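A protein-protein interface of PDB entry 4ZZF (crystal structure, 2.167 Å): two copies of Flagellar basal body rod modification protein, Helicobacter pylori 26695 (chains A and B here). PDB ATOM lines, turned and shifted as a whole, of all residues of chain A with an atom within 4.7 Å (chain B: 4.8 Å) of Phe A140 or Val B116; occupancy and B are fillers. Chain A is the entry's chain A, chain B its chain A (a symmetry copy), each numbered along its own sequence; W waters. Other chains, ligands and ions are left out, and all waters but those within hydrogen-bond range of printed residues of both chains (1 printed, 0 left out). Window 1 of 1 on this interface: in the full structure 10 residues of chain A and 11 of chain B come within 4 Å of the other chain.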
ATOM      1  N   MET A   5     -21.757 -10.303  -4.884  1.00  0.00           N
ATOM      2  CA  MET A   5     -21.726  -9.311  -5.955  1.00  0.00           C
ATOM      3  C   MET A   5     -22.758  -8.218  -5.766  1.00  0.00           C
ATOM      4  O   MET A   5     -22.591  -7.099  -6.261  1.00  0.00           O
ATOM      5  CB  MET A   5     -21.944  -9.992  -7.304  1.00  0.00           C
ATOM      6  CG  MET A   5     -20.872 -11.011  -7.620  1.00  0.00           C
ATOM      7  SD  MET A   5     -21.384 -12.229  -8.850  1.00  0.00           S
ATOM      8  CE  MET A   5     -19.837 -13.099  -9.111  1.00  0.00           C
ATOM      9  N   LYS A   8     -22.166  -4.401  -5.618  1.00  0.00           N
ATOM     10  CA  LYS A   8     -20.912  -4.071  -6.293  1.00  0.00           C
ATOM     11  C   LYS A   8     -21.235  -3.458  -7.642  1.00  0.00           C
ATOM     12  O   LYS A   8     -22.347  -3.618  -8.151  1.00  0.00           O
ATOM     13  CB  LYS A   8     -20.013  -5.304  -6.486  1.00  0.00           C
ATOM     14  CG  LYS A   8     -19.655  -6.089  -5.200  1.00  0.00           C
ATOM     15  CD  LYS A   8     -18.830  -5.259  -4.234  1.00  0.00           C
ATOM     16  CE  LYS A   8     -18.261  -6.103  -3.098  1.00  0.00           C
ATOM     17  NZ  LYS A   8     -19.312  -6.825  -2.330  1.00  0.00           N
ATOM     18  N   ILE A   9     -20.269  -2.757  -8.219  1.00  0.00           N
ATOM     19  CA  ILE A   9     -20.346  -2.406  -9.623  1.00  0.00           C
ATOM     20  C   ILE A   9     -19.748  -3.562 -10.380  1.00  0.00           C
ATOM     21  O   ILE A   9     -18.681  -4.072 -10.010  1.00  0.00           O
ATOM     22  CB  ILE A   9     -19.594  -1.097  -9.968  1.00  0.00           C
ATOM     23  CG1 ILE A   9     -20.048   0.040  -9.052  1.00  0.00           C
ATOM     24  CG2 ILE A   9     -19.777  -0.735 -11.465  1.00  0.00           C
ATOM     25  CD1 ILE A   9     -21.380   0.621  -9.428  1.00  0.00           C
ATOM     26  N   ALA A  10     -20.458  -4.004 -11.415  1.00  0.00           N
ATOM     27  CA  ALA A  10     -19.960  -5.064 -12.288  1.00  0.00           C
ATOM     28  C   ALA A  10     -19.677  -4.493 -13.672  1.00  0.00           C
ATOM     29  O   ALA A  10     -20.448  -3.675 -14.176  1.00  0.00           O
ATOM     30  CB  ALA A  10     -20.959  -6.203 -12.377  1.00  0.00           C
ATOM     31  N   VAL A 113     -24.901  -3.970  -9.234  1.00  0.00           N
ATOM     32  CA  VAL A 113     -25.674  -5.194  -9.190  1.00  0.00           C
ATOM     33  C   VAL A 113     -26.778  -5.066  -8.168  1.00  0.00           C
ATOM     34  O   VAL A 113     -26.516  -4.994  -6.972  1.00  0.00           O
ATOM     35  CB  VAL A 113     -24.807  -6.396  -8.851  1.00  0.00           C
ATOM     36  CG1 VAL A 113     -25.668  -7.658  -8.823  1.00  0.00           C
ATOM     37  CG2 VAL A 113     -23.664  -6.506  -9.862  1.00  0.00           C
ATOM     38  N   LEU A 125     -27.234 -11.864 -12.787  1.00  0.00           N
ATOM     39  CA  LEU A 125     -27.127 -10.555 -12.163  1.00  0.00           C
ATOM     40  C   LEU A 125     -28.214  -9.625 -12.675  1.00  0.00           C
ATOM     41  O   LEU A 125     -28.371  -9.462 -13.886  1.00  0.00           O
ATOM     42  CB  LEU A 125     -25.767  -9.939 -12.450  1.00  0.00           C
ATOM     43  CG  LEU A 125     -24.517 -10.721 -12.093  1.00  0.00           C
ATOM     44  CD1 LEU A 125     -23.297  -9.976 -12.658  1.00  0.00           C
ATOM     45  CD2 LEU A 125     -24.435 -10.859 -10.575  1.00  0.00           C
ATOM     46  N   ALA A 137     -19.535 -11.513 -16.452  1.00  0.00           N
ATOM     47  CA  ALA A 137     -18.889 -10.490 -15.634  1.00  0.00           C
ATOM     48  C   ALA A 137     -17.371 -10.606 -15.682  1.00  0.00           C
ATOM     49  O   ALA A 137     -16.820 -11.670 -15.401  1.00  0.00           O
ATOM     50  CB  ALA A 137     -19.367 -10.576 -14.211  1.00  0.00           C
ATOM     51  N   ILE A 138     -16.697  -9.508 -16.019  1.00  0.00           N
ATOM     52  CA  ILE A 138     -15.243  -9.529 -16.115  1.00  0.00           C
ATOM     53  C   ILE A 138     -14.542  -8.806 -14.954  1.00  0.00           C
ATOM     54  O   ILE A 138     -13.354  -9.027 -14.721  1.00  0.00           O
ATOM     55  CB  ILE A 138     -14.758  -8.915 -17.441  1.00  0.00           C
ATOM     56  CG1 ILE A 138     -15.183  -7.449 -17.566  1.00  0.00           C
ATOM     57  CG2 ILE A 138     -15.238  -9.752 -18.630  1.00  0.00           C
ATOM     58  CD1 ILE A 138     -15.006  -6.888 -19.008  1.00  0.00           C
ATOM     59  N   GLU A 139     -15.269  -7.958 -14.225  1.00  0.00           N
ATOM     60  CA  GLU A 139     -14.673  -7.223 -13.109  1.00  0.00           C
ATOM     61  C   GLU A 139     -15.720  -6.752 -12.110  1.00  0.00           C
ATOM     62  O   GLU A 139     -16.821  -6.392 -12.514  1.00  0.00           O
ATOM     63  CB  GLU A 139     -13.886  -6.009 -13.619  1.00  0.00           C
ATOM     64  CG  GLU A 139     -13.000  -5.433 -12.547  1.00  0.00           C
ATOM     65  CD  GLU A 139     -12.208  -4.217 -12.976  1.00  0.00           C
ATOM     66  OE1 GLU A 139     -12.512  -3.619 -14.037  1.00  0.00           O
ATOM     67  OE2 GLU A 139     -11.265  -3.871 -12.231  1.00  0.00           O
ATOM     68  N   PHE A 140     -15.382  -6.758 -10.815  1.00  0.00           N
ATOM     69  CA  PHE A 140     -16.228  -6.140  -9.785  1.00  0.00           C
ATOM     70  C   PHE A 140     -15.444  -5.190  -8.896  1.00  0.00           C
ATOM     71  O   PHE A 140     -14.283  -5.454  -8.566  1.00  0.00           O
ATOM     72  CB  PHE A 140     -16.890  -7.183  -8.877  1.00  0.00           C
ATOM     73  CG  PHE A 140     -17.803  -8.143  -9.588  1.00  0.00           C
ATOM     74  CD1 PHE A 140     -17.296  -9.295 -10.177  1.00  0.00           C
ATOM     75  CD2 PHE A 140     -19.175  -7.921  -9.618  1.00  0.00           C
ATOM     76  CE1 PHE A 140     -18.143 -10.198 -10.800  1.00  0.00           C
ATOM     77  CE2 PHE A 140     -20.023  -8.806 -10.241  1.00  0.00           C
ATOM     78  CZ  PHE A 140     -19.516  -9.947 -10.829  1.00  0.00           C
ATOM     79  N   TYR A 141     -16.096  -4.106  -8.482  1.00  0.00           N
ATOM     80  CA  TYR A 141     -15.520  -3.176  -7.507  1.00  0.00           C
ATOM     81  C   TYR A 141     -16.636  -2.438  -6.754  1.00  0.00           C
ATOM     82  O   TYR A 141     -17.811  -2.523  -7.119  1.00  0.00           O
ATOM     83  CB  TYR A 141     -14.557  -2.183  -8.195  1.00  0.00           C
ATOM     84  CG  TYR A 141     -15.120  -1.493  -9.413  1.00  0.00           C
ATOM     85  CD1 TYR A 141     -15.824  -0.291  -9.299  1.00  0.00           C
ATOM     86  CD2 TYR A 141     -14.940  -2.027 -10.682  1.00  0.00           C
ATOM     87  CE1 TYR A 141     -16.343   0.357 -10.425  1.00  0.00           C
ATOM     88  CE2 TYR A 141     -15.447  -1.386 -11.810  1.00  0.00           C
ATOM     89  CZ  TYR A 141     -16.150  -0.204 -11.677  1.00  0.00           C
ATOM     90  OH  TYR A 141     -16.656   0.427 -12.797  1.00  0.00           O
ATOM     91  N   SER B   2     -16.436 -16.018  -5.811  1.00  0.00           N
ATOM     92  CA  SER B   2     -16.728 -15.026  -4.782  1.00  0.00           C
ATOM     93  C   SER B   2     -15.932 -13.720  -4.958  1.00  0.00           C
ATOM     94  O   SER B   2     -14.727 -13.726  -5.245  1.00  0.00           O
ATOM     95  CB  SER B   2     -16.473 -15.617  -3.382  1.00  0.00           C
ATOM     96  OG  SER B   2     -17.015 -14.778  -2.382  1.00  0.00           O
ATOM     97  N   VAL B   3     -16.634 -12.605  -4.771  1.00  0.00           N
ATOM     98  CA  VAL B   3     -16.035 -11.285  -4.777  1.00  0.00           C
ATOM     99  C   VAL B   3     -16.079 -10.656  -3.370  1.00  0.00           C
ATOM    100  O   VAL B   3     -15.947  -9.436  -3.214  1.00  0.00           O
ATOM    101  CB  VAL B   3     -16.735 -10.348  -5.817  1.00  0.00           C
ATOM    102  CG1 VAL B   3     -16.823 -11.041  -7.169  1.00  0.00           C
ATOM    103  CG2 VAL B   3     -18.124  -9.886  -5.355  1.00  0.00           C
ATOM    104  N   ILE B   6     -13.227  -8.212  -2.019  1.00  0.00           N
ATOM    105  CA  ILE B   6     -13.178  -6.794  -2.316  1.00  0.00           C
ATOM    106  C   ILE B   6     -13.403  -5.986  -1.046  1.00  0.00           C
ATOM    107  O   ILE B   6     -14.350  -6.231  -0.318  1.00  0.00           O
ATOM    108  CB  ILE B   6     -14.219  -6.408  -3.362  1.00  0.00           C
ATOM    109  CG1 ILE B   6     -13.871  -7.045  -4.710  1.00  0.00           C
ATOM    110  CG2 ILE B   6     -14.319  -4.892  -3.478  1.00  0.00           C
ATOM    111  CD1 ILE B   6     -15.000  -6.951  -5.696  1.00  0.00           C
ATOM    112  N   VAL B 113      -7.881  -5.000  -1.224  1.00  0.00           N
ATOM    113  CA  VAL B 113      -8.313  -5.504  -2.511  1.00  0.00           C
ATOM    114  C   VAL B 113      -9.273  -4.527  -3.147  1.00  0.00           C
ATOM    115  O   VAL B 113     -10.385  -4.340  -2.663  1.00  0.00           O
ATOM    116  CB  VAL B 113      -8.981  -6.865  -2.390  1.00  0.00           C
ATOM    117  CG1 VAL B 113      -9.411  -7.351  -3.772  1.00  0.00           C
ATOM    118  CG2 VAL B 113      -8.025  -7.847  -1.710  1.00  0.00           C
ATOM    119  N   GLU B 114      -8.847  -3.903  -4.238  1.00  0.00           N
ATOM    120  CA  GLU B 114      -9.621  -2.829  -4.835  1.00  0.00           C
ATOM    121  C   GLU B 114     -10.643  -3.329  -5.850  1.00  0.00           C
ATOM    122  O   GLU B 114     -11.656  -2.679  -6.095  1.00  0.00           O
ATOM    123  CB  GLU B 114      -8.684  -1.822  -5.493  1.00  0.00           C
ATOM    124  CG  GLU B 114      -7.718  -1.189  -4.507  1.00  0.00           C
ATOM    125  CD  GLU B 114      -6.752  -0.241  -5.173  1.00  0.00           C
ATOM    126  OE1 GLU B 114      -5.976  -0.702  -6.036  1.00  0.00           O
ATOM    127  OE2 GLU B 114      -6.777   0.963  -4.840  1.00  0.00           O
ATOM    128  N   SER B 115     -10.380  -4.479  -6.452  1.00  0.00           N
ATOM    129  CA  SER B 115     -11.350  -5.063  -7.360  1.00  0.00           C
ATOM    130  C   SER B 115     -10.987  -6.510  -7.569  1.00  0.00           C
ATOM    131  O   SER B 115      -9.875  -6.921  -7.267  1.00  0.00           O
ATOM    132  CB  SER B 115     -11.398  -4.305  -8.700  1.00  0.00           C
ATOM    133  OG  SER B 115     -10.368  -4.715  -9.575  1.00  0.00           O
ATOM    134  N   VAL B 116     -11.946  -7.286  -8.055  1.00  0.00           N
ATOM    135  CA  VAL B 116     -11.696  -8.649  -8.499  1.00  0.00           C
ATOM    136  C   VAL B 116     -11.909  -8.696  -9.998  1.00  0.00           C
ATOM    137  O   VAL B 116     -12.941  -8.258 -10.493  1.00  0.00           O
ATOM    138  CB  VAL B 116     -12.610  -9.673  -7.797  1.00  0.00           C
ATOM    139  CG1 VAL B 116     -12.599 -11.010  -8.541  1.00  0.00           C
ATOM    140  CG2 VAL B 116     -12.177  -9.862  -6.366  1.00  0.00           C
ATOM    141  N   ILE B 117     -10.917  -9.208 -10.712  1.00  0.00           N
ATOM    142  CA  ILE B 117     -10.962  -9.295 -12.158  1.00  0.00           C
ATOM    143  C   ILE B 117     -11.064 -10.737 -12.596  1.00  0.00           C
ATOM    144  O   ILE B 117     -10.335 -11.590 -12.093  1.00  0.00           O
ATOM    145  CB  ILE B 117      -9.706  -8.700 -12.796  1.00  0.00           C
ATOM    146  CG1 ILE B 117      -9.574  -7.230 -12.440  1.00  0.00           C
ATOM    147  CG2 ILE B 117      -9.727  -8.898 -14.308  1.00  0.00           C
ATOM    148  CD1 ILE B 117      -8.260  -6.656 -12.879  1.00  0.00           C
ATOM    149  N   PHE B 118     -11.954 -11.025 -13.535  1.00  0.00           N
ATOM    150  CA  PHE B 118     -12.035 -12.390 -14.031  1.00  0.00           C
ATOM    151  C   PHE B 118     -11.306 -12.532 -15.347  1.00  0.00           C
ATOM    152  O   PHE B 118     -11.663 -11.941 -16.363  1.00  0.00           O
ATOM    153  CB  PHE B 118     -13.481 -12.845 -14.114  1.00  0.00           C
ATOM    154  CG  PHE B 118     -14.065 -13.080 -12.770  1.00  0.00           C
ATOM    155  CD1 PHE B 118     -13.862 -14.287 -12.127  1.00  0.00           C
ATOM    156  CD2 PHE B 118     -14.728 -12.063 -12.100  1.00  0.00           C
ATOM    157  CE1 PHE B 118     -14.360 -14.501 -10.859  1.00  0.00           C
ATOM    158  CE2 PHE B 118     -15.227 -12.262 -10.829  1.00  0.00           C
ATOM    159  CZ  PHE B 118     -15.045 -13.484 -10.204  1.00  0.00           C
ATOM    160  N   PRO B 123     -10.089 -15.932 -11.427  1.00  0.00           N
ATOM    161  CA  PRO B 123     -10.164 -14.744 -10.574  1.00  0.00           C
ATOM    162  C   PRO B 123      -8.782 -14.168 -10.245  1.00  0.00           C
ATOM    163  O   PRO B 123      -7.860 -14.905  -9.884  1.00  0.00           O
ATOM    164  CB  PRO B 123     -10.868 -15.260  -9.305  1.00  0.00           C
ATOM    165  CG  PRO B 123     -11.418 -16.610  -9.658  1.00  0.00           C
ATOM    166  CD  PRO B 123     -10.502 -17.150 -10.717  1.00  0.00           C
ATOM    167  N   MET B 124      -8.663 -12.852 -10.401  1.00  0.00           N
ATOM    168  CA  MET B 124      -7.484 -12.090 -10.006  1.00  0.00           C
ATOM    169  C   MET B 124      -7.865 -10.995  -9.008  1.00  0.00           C
ATOM    170  O   MET B 124      -8.955 -10.431  -9.074  1.00  0.00           O
ATOM    171  CB  MET B 124      -6.816 -11.448 -11.226  1.00  0.00           C
ATOM    172  CG  MET B 124      -6.664 -12.380 -12.405  1.00  0.00           C
ATOM    173  SD  MET B 124      -5.379 -13.603 -12.119  1.00  0.00           S
ATOM    174  CE  MET B 124      -3.933 -12.578 -12.357  1.00  0.00           C
ATOM    175  N   LEU B 125      -6.951 -10.679  -8.100  1.00  0.00           N
ATOM    176  CA  LEU B 125      -7.145  -9.568  -7.182  1.00  0.00           C
ATOM    177  C   LEU B 125      -6.400  -8.335  -7.665  1.00  0.00           C
ATOM    178  O   LEU B 125      -5.201  -8.402  -7.940  1.00  0.00           O
ATOM    179  CB  LEU B 125      -6.653  -9.935  -5.792  1.00  0.00           C
ATOM    180  CG  LEU B 125      -7.200 -11.183  -5.124  1.00  0.00           C
ATOM    181  CD1 LEU B 125      -6.408 -11.434  -3.833  1.00  0.00           C
ATOM    182  CD2 LEU B 125      -8.686 -10.980  -4.839  1.00  0.00           C
HETATM  183  O   HOH W   1     -17.009  -7.545  -0.375  1.00  0.00           O
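The backbone NH (N) of Phe A140 is in hydrogen-bond range of the backbone carbonyl oxygen (O) of Val B116 (2.9 Å). N of Phe B118 sits at hydrogen-bond distance from O of Ile A138. The side-chain carboxylate (OE2) of Glu A139 sits at hydrogen-bond distance from the side-chain hydroxyl (OG) of Ser B115 (2.9 Å).
The backbone NH of Met B124 lies within hydrogen-bond range of the backbone carbonyl oxygen of Ile B117 (2.7 Å). The backbone carbonyl oxygen (O) of Tyr A141 is in hydrogen-bond range of the backbone NH (N) of Ile A9.
Among the printed residues, merely in contact across the chains: Met A5 with Val B3 (3.7 Å), Ala A137 with Phe B118 (3.8 Å), Ile A138 with Ile B117 (3.5 Å), Glu A139 with Val B116 (3.3 Å), Glu A139 with Ile B117 (3.8 Å), Phe A140 with Val B3 (3.5 Å), Phe A140 with Ile B6 (3.3 Å), Phe A140 with Ser B115 (3.1 Å), Phe A140 with Phe B118 (3.6 Å), Tyr A141 with Glu B114 (3.6 Å) and Tyr A141 with Ser B115 (3.8 Å).
Leu A125 touches none of the printed residues of chain B. Printed residues of chain B within 4 Å of Ile A138: Ile B117 and Phe B118. Of chain B, only Val B3 (3.5 Å), Ile B6 (3.3 Å), Ser B115 (3.1 Å), Val B116 (2.9 Å) and Phe B118 (3.6 Å) come within 4 Å of Phe A140. Of the printed residues of chain A, Glu B114 touches Tyr A141. Printed residues of chain A within 4 Å of Ser B115: Glu A139 (2.9 Å), Phe A140 (3.1 Å) and Tyr A141 (3.8 Å). Val B116 touches two residues of chain A. Printed residues of chain A within 4 Å of Ile B117: Ile A138 and Glu A139. The nearest residue of chain A that does not touch Val B116 is Ile A138 (4.3 Å). The nearest printed residue of chain B that does not touch Met A5 is Phe B118 (4.9 Å).
Hydrophobic or aromatic side chains of chain A within 4 Å of the printed part of chain B: Met A5, Phe A140 and Tyr A141. Among the printed residues, 14 pairs touch across the chains. Among the printed residues, no Asp or Glu carboxylate lies within 4 Å of a Lys or Arg side-chain nitrogen of the other chain.
Positions printed for both chains: 113 and 125.
Water W1 lies within hydrogen-bond range of the backbone carbonyl oxygen of Ile B6 and the side-chain amino group of Lys A8.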
